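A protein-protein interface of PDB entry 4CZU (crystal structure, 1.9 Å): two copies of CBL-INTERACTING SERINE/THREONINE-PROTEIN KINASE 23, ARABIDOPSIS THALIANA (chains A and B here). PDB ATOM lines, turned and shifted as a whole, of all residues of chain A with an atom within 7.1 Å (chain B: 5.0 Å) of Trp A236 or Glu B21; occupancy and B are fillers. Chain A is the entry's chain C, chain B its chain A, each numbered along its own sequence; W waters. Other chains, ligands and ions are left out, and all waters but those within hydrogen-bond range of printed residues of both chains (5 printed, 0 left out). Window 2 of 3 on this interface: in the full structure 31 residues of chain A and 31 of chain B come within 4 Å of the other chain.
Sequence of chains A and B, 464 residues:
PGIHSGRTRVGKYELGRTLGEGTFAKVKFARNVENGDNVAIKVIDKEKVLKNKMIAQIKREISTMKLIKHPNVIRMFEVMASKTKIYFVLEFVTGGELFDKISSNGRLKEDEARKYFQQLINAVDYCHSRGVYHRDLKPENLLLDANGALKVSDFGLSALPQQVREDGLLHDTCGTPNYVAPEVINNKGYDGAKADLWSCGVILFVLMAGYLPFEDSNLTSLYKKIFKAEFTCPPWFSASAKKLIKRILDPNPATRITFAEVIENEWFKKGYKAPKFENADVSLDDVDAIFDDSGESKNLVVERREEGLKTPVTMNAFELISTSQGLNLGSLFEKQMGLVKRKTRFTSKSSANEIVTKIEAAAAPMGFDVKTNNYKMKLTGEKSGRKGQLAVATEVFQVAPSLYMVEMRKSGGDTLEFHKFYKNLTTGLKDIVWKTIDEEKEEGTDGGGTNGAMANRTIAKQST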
ATOM      1  N   GLY A 106       8.269   2.523   7.160  1.00  0.00           N
ATOM      2  CA  GLY A 106       9.233   1.469   6.880  1.00  0.00           C
ATOM      3  C   GLY A 106       8.824   0.132   7.464  1.00  0.00           C
ATOM      4  O   GLY A 106       7.675  -0.063   7.875  1.00  0.00           O
ATOM      5  N   ARG A 107       9.763  -0.808   7.507  1.00  0.00           N
ATOM      6  CA  ARG A 107       9.449  -2.177   7.919  1.00  0.00           C
ATOM      7  C   ARG A 107       8.895  -2.231   9.346  1.00  0.00           C
ATOM      8  O   ARG A 107       9.251  -1.399  10.185  1.00  0.00           O
ATOM      9  CB  ARG A 107      10.702  -3.043   7.826  1.00  0.00           C
ATOM     10  CG  ARG A 107      11.810  -2.672   8.824  1.00  0.00           C
ATOM     11  CD  ARG A 107      12.941  -3.684   8.702  1.00  0.00           C
ATOM     12  NE  ARG A 107      14.005  -3.541   9.703  1.00  0.00           N
ATOM     13  CZ  ARG A 107      15.195  -3.002   9.454  1.00  0.00           C
ATOM     14  NH1 ARG A 107      15.469  -2.531   8.246  1.00  0.00           N
ATOM     15  NH2 ARG A 107      16.112  -2.926  10.414  1.00  0.00           N
ATOM     16  N   LEU A 108       8.027  -3.205   9.625  1.00  0.00           N
ATOM     17  CA  LEU A 108       7.525  -3.388  10.991  1.00  0.00           C
ATOM     18  C   LEU A 108       8.546  -4.145  11.828  1.00  0.00           C
ATOM     19  O   LEU A 108       9.360  -4.894  11.294  1.00  0.00           O
ATOM     20  CB  LEU A 108       6.227  -4.200  11.017  1.00  0.00           C
ATOM     21  CG  LEU A 108       5.035  -3.964  10.089  1.00  0.00           C
ATOM     22  CD1 LEU A 108       3.790  -4.717  10.652  1.00  0.00           C
ATOM     23  CD2 LEU A 108       4.735  -2.506   9.819  1.00  0.00           C
ATOM     24  N   GLU A 110       9.778  -7.171  14.257  1.00  0.00           N
ATOM     25  CA  GLU A 110       9.455  -8.592  14.135  1.00  0.00           C
ATOM     26  C   GLU A 110       8.187  -9.002  14.879  1.00  0.00           C
ATOM     27  O   GLU A 110       7.361  -9.743  14.342  1.00  0.00           O
ATOM     28  CB  GLU A 110      10.615  -9.469  14.592  1.00  0.00           C
ATOM     29  CG  GLU A 110      10.294 -10.942  14.471  1.00  0.00           C
ATOM     30  CD  GLU A 110      11.440 -11.837  14.883  1.00  0.00           C
ATOM     31  OE1 GLU A 110      11.901 -11.727  16.048  1.00  0.00           O
ATOM     32  OE2 GLU A 110      11.882 -12.651  14.038  1.00  0.00           O
ATOM     33  N   PHE A 205       7.122 -11.624   4.294  1.00  0.00           N
ATOM     34  CA  PHE A 205       8.426 -11.070   3.869  1.00  0.00           C
ATOM     35  C   PHE A 205       8.410  -9.548   3.803  1.00  0.00           C
ATOM     36  O   PHE A 205       9.301  -8.888   4.361  1.00  0.00           O
ATOM     37  CB  PHE A 205       8.891 -11.665   2.524  1.00  0.00           C
ATOM     38  CG  PHE A 205      10.307 -11.272   2.145  1.00  0.00           C
ATOM     39  CD1 PHE A 205      10.589 -10.024   1.609  1.00  0.00           C
ATOM     40  CD2 PHE A 205      11.338 -12.161   2.328  1.00  0.00           C
ATOM     41  CE1 PHE A 205      11.897  -9.673   1.266  1.00  0.00           C
ATOM     42  CE2 PHE A 205      12.632 -11.823   1.973  1.00  0.00           C
ATOM     43  CZ  PHE A 205      12.906 -10.572   1.451  1.00  0.00           C
ATOM     44  N   LEU A 207       6.357  -7.347   5.177  1.00  0.00           N
ATOM     45  CA  LEU A 207       6.171  -6.708   6.486  1.00  0.00           C
ATOM     46  C   LEU A 207       7.491  -6.647   7.255  1.00  0.00           C
ATOM     47  O   LEU A 207       7.791  -5.648   7.909  1.00  0.00           O
ATOM     48  CB  LEU A 207       5.149  -7.481   7.320  1.00  0.00           C
ATOM     49  CG  LEU A 207       3.686  -7.388   6.850  1.00  0.00           C
ATOM     50  CD1 LEU A 207       2.855  -8.433   7.583  1.00  0.00           C
ATOM     51  CD2 LEU A 207       3.118  -5.987   7.062  1.00  0.00           C
ATOM     52  N   MET A 208       8.269  -7.724   7.183  1.00  0.00           N
ATOM     53  CA  MET A 208       9.513  -7.811   7.938  1.00  0.00           C
ATOM     54  C   MET A 208      10.703  -7.167   7.242  1.00  0.00           C
ATOM     55  O   MET A 208      11.665  -6.803   7.911  1.00  0.00           O
ATOM     56  CB  MET A 208       9.860  -9.268   8.252  1.00  0.00           C
ATOM     57  CG  MET A 208       8.960  -9.890   9.290  1.00  0.00           C
ATOM     58  SD  MET A 208       9.389 -11.591   9.605  1.00  0.00           S
ATOM     59  CE  MET A 208      10.875 -11.415  10.587  1.00  0.00           C
ATOM     60  N   ALA A 209      10.654  -7.067   5.911  1.00  0.00           N
ATOM     61  CA  ALA A 209      11.747  -6.454   5.146  1.00  0.00           C
ATOM     62  C   ALA A 209      11.467  -5.010   4.742  1.00  0.00           C
ATOM     63  O   ALA A 209      12.387  -4.184   4.659  1.00  0.00           O
ATOM     64  CB  ALA A 209      12.089  -7.309   3.898  1.00  0.00           C
ATOM     65  N   GLY A 210      10.200  -4.697   4.481  1.00  0.00           N
ATOM     66  CA  GLY A 210       9.841  -3.408   3.925  1.00  0.00           C
ATOM     67  C   GLY A 210       9.964  -3.324   2.409  1.00  0.00           C
ATOM     68  O   GLY A 210       9.774  -2.262   1.829  1.00  0.00           O
ATOM     69  N   TYR A 211      10.264  -4.443   1.754  1.00  0.00           N
ATOM     70  CA  TYR A 211      10.370  -4.447   0.300  1.00  0.00           C
ATOM     71  C   TYR A 211      10.056  -5.829  -0.215  1.00  0.00           C
ATOM     72  O   TYR A 211      10.030  -6.777   0.550  1.00  0.00           O
ATOM     73  CB  TYR A 211      11.762  -3.984  -0.191  1.00  0.00           C
ATOM     74  CG  TYR A 211      12.927  -4.717   0.423  1.00  0.00           C
ATOM     75  CD1 TYR A 211      13.340  -5.951  -0.078  1.00  0.00           C
ATOM     76  CD2 TYR A 211      13.631  -4.173   1.493  1.00  0.00           C
ATOM     77  CE1 TYR A 211      14.412  -6.631   0.480  1.00  0.00           C
ATOM     78  CE2 TYR A 211      14.713  -4.852   2.065  1.00  0.00           C
ATOM     79  CZ  TYR A 211      15.097  -6.074   1.553  1.00  0.00           C
ATOM     80  OH  TYR A 211      16.160  -6.752   2.109  1.00  0.00           O
ATOM     81  N   CYS A 233      16.910 -13.080   2.089  1.00  0.00           N
ATOM     82  CA  CYS A 233      16.419 -12.482   3.329  1.00  0.00           C
ATOM     83  C   CYS A 233      17.418 -11.463   3.866  1.00  0.00           C
ATOM     84  O   CYS A 233      18.625 -11.707   3.835  1.00  0.00           O
ATOM     85  CB  CYS A 233      16.151 -13.560   4.369  1.00  0.00           C
ATOM     86  SG  CYS A 233      14.781 -14.635   3.899  1.00  0.00           S
ATOM     87  N   PRO A 234      16.927 -10.314   4.349  1.00  0.00           N
ATOM     88  CA  PRO A 234      17.882  -9.332   4.872  1.00  0.00           C
ATOM     89  C   PRO A 234      18.531  -9.816   6.185  1.00  0.00           C
ATOM     90  O   PRO A 234      18.059 -10.776   6.804  1.00  0.00           O
ATOM     91  CB  PRO A 234      17.029  -8.069   5.072  1.00  0.00           C
ATOM     92  CG  PRO A 234      15.629  -8.553   5.165  1.00  0.00           C
ATOM     93  CD  PRO A 234      15.544  -9.801   4.321  1.00  0.00           C
ATOM     94  N   PRO A 235      19.643  -9.183   6.590  1.00  0.00           N
ATOM     95  CA  PRO A 235      20.400  -9.691   7.744  1.00  0.00           C
ATOM     96  C   PRO A 235      19.667  -9.579   9.087  1.00  0.00           C
ATOM     97  O   PRO A 235      20.010 -10.299  10.030  1.00  0.00           O
ATOM     98  CB  PRO A 235      21.690  -8.843   7.726  1.00  0.00           C
ATOM     99  CG  PRO A 235      21.358  -7.651   6.920  1.00  0.00           C
ATOM    100  CD  PRO A 235      20.352  -8.101   5.891  1.00  0.00           C
ATOM    101  N   TRP A 236      18.652  -8.720   9.164  1.00  0.00           N
ATOM    102  CA  TRP A 236      17.886  -8.557  10.405  1.00  0.00           C
ATOM    103  C   TRP A 236      16.851  -9.665  10.638  1.00  0.00           C
ATOM    104  O   TRP A 236      16.282  -9.763  11.733  1.00  0.00           O
ATOM    105  CB  TRP A 236      17.241  -7.162  10.488  1.00  0.00           C
ATOM    106  CG  TRP A 236      16.309  -6.799   9.347  1.00  0.00           C
ATOM    107  CD1 TRP A 236      14.994  -7.152   9.221  1.00  0.00           C
ATOM    108  CD2 TRP A 236      16.622  -5.997   8.195  1.00  0.00           C
ATOM    109  NE1 TRP A 236      14.465  -6.620   8.056  1.00  0.00           N
ATOM    110  CE2 TRP A 236      15.447  -5.911   7.412  1.00  0.00           C
ATOM    111  CE3 TRP A 236      17.782  -5.346   7.750  1.00  0.00           C
ATOM    112  CZ2 TRP A 236      15.400  -5.208   6.207  1.00  0.00           C
ATOM    113  CZ3 TRP A 236      17.735  -4.646   6.555  1.00  0.00           C
ATOM    114  CH2 TRP A 236      16.545  -4.573   5.796  1.00  0.00           C
ATOM    115  N   PHE A 237      16.602 -10.497   9.624  1.00  0.00           N
ATOM    116  CA  PHE A 237      15.730 -11.659   9.816  1.00  0.00           C
ATOM    117  C   PHE A 237      16.429 -12.638  10.751  1.00  0.00           C
ATOM    118  O   PHE A 237      17.614 -12.934  10.591  1.00  0.00           O
ATOM    119  CB  PHE A 237      15.439 -12.410   8.496  1.00  0.00           C
ATOM    120  CG  PHE A 237      14.340 -11.799   7.644  1.00  0.00           C
ATOM    121  CD1 PHE A 237      13.997 -10.463   7.751  1.00  0.00           C
ATOM    122  CD2 PHE A 237      13.660 -12.592   6.717  1.00  0.00           C
ATOM    123  CE1 PHE A 237      13.000  -9.926   6.949  1.00  0.00           C
ATOM    124  CE2 PHE A 237      12.667 -12.064   5.921  1.00  0.00           C
ATOM    125  CZ  PHE A 237      12.331 -10.723   6.038  1.00  0.00           C
ATOM    126  N   SER A 238      15.682 -13.184  11.704  1.00  0.00           N
ATOM    127  CA  SER A 238      16.221 -14.251  12.545  1.00  0.00           C
ATOM    128  C   SER A 238      16.379 -15.554  11.773  1.00  0.00           C
ATOM    129  O   SER A 238      15.765 -15.753  10.718  1.00  0.00           O
ATOM    130  CB  SER A 238      15.305 -14.496  13.747  1.00  0.00           C
ATOM    131  OG  SER A 238      14.160 -15.234  13.356  1.00  0.00           O
ATOM    132  N   ALA A 239      17.188 -16.458  12.320  1.00  0.00           N
ATOM    133  CA  ALA A 239      17.424 -17.740  11.683  1.00  0.00           C
ATOM    134  C   ALA A 239      16.111 -18.513  11.538  1.00  0.00           C
ATOM    135  O   ALA A 239      15.828 -19.113  10.490  1.00  0.00           O
ATOM    136  CB  ALA A 239      18.428 -18.541  12.491  1.00  0.00           C
ATOM    137  N   ALA A 241      12.960 -17.322  11.515  1.00  0.00           N
ATOM    138  CA  ALA A 241      12.013 -16.686  10.599  1.00  0.00           C
ATOM    139  C   ALA A 241      12.403 -16.936   9.142  1.00  0.00           C
ATOM    140  O   ALA A 241      11.557 -17.260   8.311  1.00  0.00           O
ATOM    141  CB  ALA A 241      11.919 -15.205  10.863  1.00  0.00           C
ATOM    142  N   THR B  18      16.472   7.189  10.603  1.00  0.00           N
ATOM    143  CA  THR B  18      16.123   6.471   9.395  1.00  0.00           C
ATOM    144  C   THR B  18      14.622   6.215   9.330  1.00  0.00           C
ATOM    145  O   THR B  18      14.031   5.636  10.243  1.00  0.00           O
ATOM    146  CB  THR B  18      16.864   5.134   9.345  1.00  0.00           C
ATOM    147  OG1 THR B  18      18.275   5.376   9.412  1.00  0.00           O
ATOM    148  CG2 THR B  18      16.542   4.388   8.067  1.00  0.00           C
ATOM    149  N   LEU B  19      14.011   6.667   8.240  1.00  0.00           N
ATOM    150  CA  LEU B  19      12.617   6.410   7.965  1.00  0.00           C
ATOM    151  C   LEU B  19      12.467   5.032   7.316  1.00  0.00           C
ATOM    152  O   LEU B  19      11.659   4.214   7.758  1.00  0.00           O
ATOM    153  CB  LEU B  19      12.102   7.486   7.023  1.00  0.00           C
ATOM    154  CG  LEU B  19      10.649   7.396   6.549  1.00  0.00           C
ATOM    155  CD1 LEU B  19       9.681   7.701   7.685  1.00  0.00           C
ATOM    156  CD2 LEU B  19      10.426   8.344   5.376  1.00  0.00           C
ATOM    157  N   GLY B  20      13.252   4.783   6.265  1.00  0.00           N
ATOM    158  CA  GLY B  20      13.216   3.517   5.553  1.00  0.00           C
ATOM    159  C   GLY B  20      14.605   3.004   5.215  1.00  0.00           C
ATOM    160  O   GLY B  20      15.524   3.778   4.968  1.00  0.00           O
ATOM    161  N   GLU B  21      14.759   1.690   5.185  1.00  0.00           N
ATOM    162  CA  GLU B  21      16.029   1.112   4.805  1.00  0.00           C
ATOM    163  C   GLU B  21      15.837   0.004   3.776  1.00  0.00           C
ATOM    164  O   GLU B  21      15.041  -0.918   3.983  1.00  0.00           O
ATOM    165  CB  GLU B  21      16.761   0.574   6.037  1.00  0.00           C
ATOM    166  CG  GLU B  21      18.018  -0.225   5.718  1.00  0.00           C
ATOM    167  CD  GLU B  21      18.598  -0.926   6.939  1.00  0.00           C
ATOM    168  OE1 GLU B  21      17.902  -1.012   7.976  1.00  0.00           O
ATOM    169  OE2 GLU B  21      19.755  -1.398   6.867  1.00  0.00           O
ATOM    170  N   GLY B  22      16.561   0.112   2.667  1.00  0.00           N
ATOM    171  CA  GLY B  22      16.648  -0.958   1.701  1.00  0.00           C
ATOM    172  C   GLY B  22      18.043  -1.564   1.794  1.00  0.00           C
ATOM    173  O   GLY B  22      18.779  -1.286   2.742  1.00  0.00           O
ATOM    174  N   THR B  23      18.413  -2.372   0.800  1.00  0.00           N
ATOM    175  CA  THR B  23      19.717  -3.024   0.769  1.00  0.00           C
ATOM    176  C   THR B  23      20.861  -2.048   0.507  1.00  0.00           C
ATOM    177  O   THR B  23      21.935  -2.183   1.088  1.00  0.00           O
ATOM    178  CB  THR B  23      19.744  -4.119  -0.312  1.00  0.00           C
ATOM    179  OG1 THR B  23      18.707  -5.063  -0.031  1.00  0.00           O
ATOM    180  CG2 THR B  23      21.078  -4.840  -0.310  1.00  0.00           C
ATOM    181  N   ALA B  25      20.209   1.593  -0.048  1.00  0.00           N
ATOM    182  CA  ALA B  25      19.759   2.973   0.137  1.00  0.00           C
ATOM    183  C   ALA B  25      18.949   3.096   1.423  1.00  0.00           C
ATOM    184  O   ALA B  25      18.348   2.131   1.871  1.00  0.00           O
ATOM    185  CB  ALA B  25      18.912   3.386  -1.047  1.00  0.00           C
ATOM    186  N   LYS B  26      18.946   4.287   2.018  1.00  0.00           N
ATOM    187  CA  LYS B  26      18.138   4.566   3.196  1.00  0.00           C
ATOM    188  C   LYS B  26      17.534   5.927   2.980  1.00  0.00           C
ATOM    189  O   LYS B  26      18.082   6.724   2.230  1.00  0.00           O
ATOM    190  CB  LYS B  26      19.021   4.640   4.444  1.00  0.00           C
ATOM    191  CG  LYS B  26      19.434   3.323   5.009  1.00  0.00           C
ATOM    192  CD  LYS B  26      20.384   3.563   6.173  1.00  0.00           C
ATOM    193  CE  LYS B  26      20.892   2.258   6.748  1.00  0.00           C
ATOM    194  NZ  LYS B  26      21.818   2.529   7.883  1.00  0.00           N
ATOM    195  N   GLU B 166      16.072   1.103  -4.031  1.00  0.00           N
ATOM    196  CA  GLU B 166      15.097   0.558  -3.075  1.00  0.00           C
ATOM    197  C   GLU B 166      15.395   0.990  -1.633  1.00  0.00           C
ATOM    198  O   GLU B 166      16.461   0.691  -1.100  1.00  0.00           O
ATOM    199  CB  GLU B 166      15.042  -0.978  -3.180  1.00  0.00           C
ATOM    200  CG  GLU B 166      14.017  -1.641  -2.244  1.00  0.00           C
ATOM    201  CD  GLU B 166      12.629  -1.034  -2.370  1.00  0.00           C
ATOM    202  OE1 GLU B 166      12.045  -1.065  -3.482  1.00  0.00           O
ATOM    203  OE2 GLU B 166      12.107  -0.510  -1.357  1.00  0.00           O
ATOM    204  N   ASP B 167      14.443   1.696  -1.018  1.00  0.00           N
ATOM    205  CA  ASP B 167      14.638   2.304   0.298  1.00  0.00           C
ATOM    206  C   ASP B 167      13.778   1.748   1.430  1.00  0.00           C
ATOM    207  O   ASP B 167      13.751   2.326   2.521  1.00  0.00           O
ATOM    208  CB  ASP B 167      14.431   3.822   0.223  1.00  0.00           C
ATOM    209  CG  ASP B 167      13.091   4.205  -0.399  1.00  0.00           C
ATOM    210  OD1 ASP B 167      12.156   3.373  -0.402  1.00  0.00           O
ATOM    211  OD2 ASP B 167      12.963   5.342  -0.900  1.00  0.00           O
ATOM    212  N   GLY B 168      13.073   0.646   1.176  1.00  0.00           N
ATOM    213  CA  GLY B 168      12.231   0.030   2.184  1.00  0.00           C
ATOM    214  C   GLY B 168      10.944   0.782   2.486  1.00  0.00           C
ATOM    215  O   GLY B 168      10.396   0.632   3.574  1.00  0.00           O
HETATM  216  O   HOH W   1       9.641  -1.469  -0.653  1.00  0.00           O
HETATM  217  O   HOH W   2      13.624  -2.133   5.734  1.00  0.00           O
HETATM  218  O   HOH W   3      18.909  -5.751   2.714  1.00  0.00           O
HETATM  219  O   HOH W   4      11.956   0.082   5.881  1.00  0.00           O
HETATM  220  O   HOH W   5      18.881  -2.444  10.518  1.00  0.00           O
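No position is printed for both chains.
The side-chain carboxylate of Glu B21 lies within salt-bridge range of the guanidinium group of Arg A107, 2.9 Å away. The backbone carbonyl oxygen (O) of Gly B168 lies close to the backbone carbonyl oxygen (O) of Gly A210, at 3.4 Å.
The backbone NH (N) of Glu B21 lies within hydrogen-bond range of the backbone carbonyl oxygen (O) of Asp B167, at 2.9 Å. The side-chain carboxylate (OE2) of Glu B166 is in hydrogen-bond range of the backbone NH (N) of Gly B168, 2.9 Å away. The backbone carbonyl oxygen of Met A208 is in hydrogen-bond range of the indole nitrogen of Trp A236, at 2.8 Å.
Among the printed residues, pairs that only touch across the chains: Gly A106 with Leu B19 (3.8 Å), Gly A106 with Gly B168 (3.6 Å), Tyr A211 with Thr B23 (3.7 Å), Tyr A211 with Glu B166 (3.7 Å) and Trp A236 with Glu B21 (3.8 Å).
Of the printed residues of chain B, Gly A106 touches Leu B19 (3.8 Å) and Gly B168 (3.6 Å). Ala A209 touches none of the printed residues of chain B. Printed residues of chain B within 4 Å of Tyr A211: Thr B23 and Glu B166. Printed residues of chain B within 4 Å of Trp A236: Glu B21. Glu B21 touches just these residues of chain A: Arg A107 (2.9 Å) and Trp A236 (3.8 Å). Of the printed residues of chain A, Thr B23 touches Tyr A211. Printed residues of chain A within 4 Å of Gly B168: Gly A106 and Gly A210. The nearest printed residue of chain B that does not touch Trp A236 is Gly B22 (5.0 Å).
Along chain B the printed residues that touch a printed residue of chain A span positions 19 to 168. Printed residues of chain A that touch a printed residue of chain B: Gly A106, Arg A107, Gly A210, Tyr A211 and Trp A236. Hydrophobic or aromatic side chains of chain A that line the printed part of chain B: Tyr A211 and Trp A236. Among the printed residues, Asp or Glu carboxylates within 4 Å of a Lys or Arg side-chain nitrogen of the other chain: Arg A107 with Glu B21 (2.9 Å).
Water W2 lies within hydrogen-bond range of the backbone carbonyl oxygen (O) of Glu B21, the backbone carbonyl oxygen (O) of Ala A209 and the guanidinium group (NH1) of Arg A107. Water W1 bridges the backbone carbonyl oxygen (O) of Gly A210 (2.6 Å) and the side-chain carboxylate (OE2) of Glu B166 (2.7 Å). Water W5 bridges the guanidinium group of Arg A107 (2.8 Å) and the side-chain carboxylate of Glu B21 (3.1 Å). Water W3 lies within hydrogen-bond range of OG1 of Thr B23 (2.8 Å) and OH of Tyr A211 (3.0 Å). Water W4 lies within hydrogen-bond range of O of Gly B168, N of Arg A107 and N of Glu B21.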
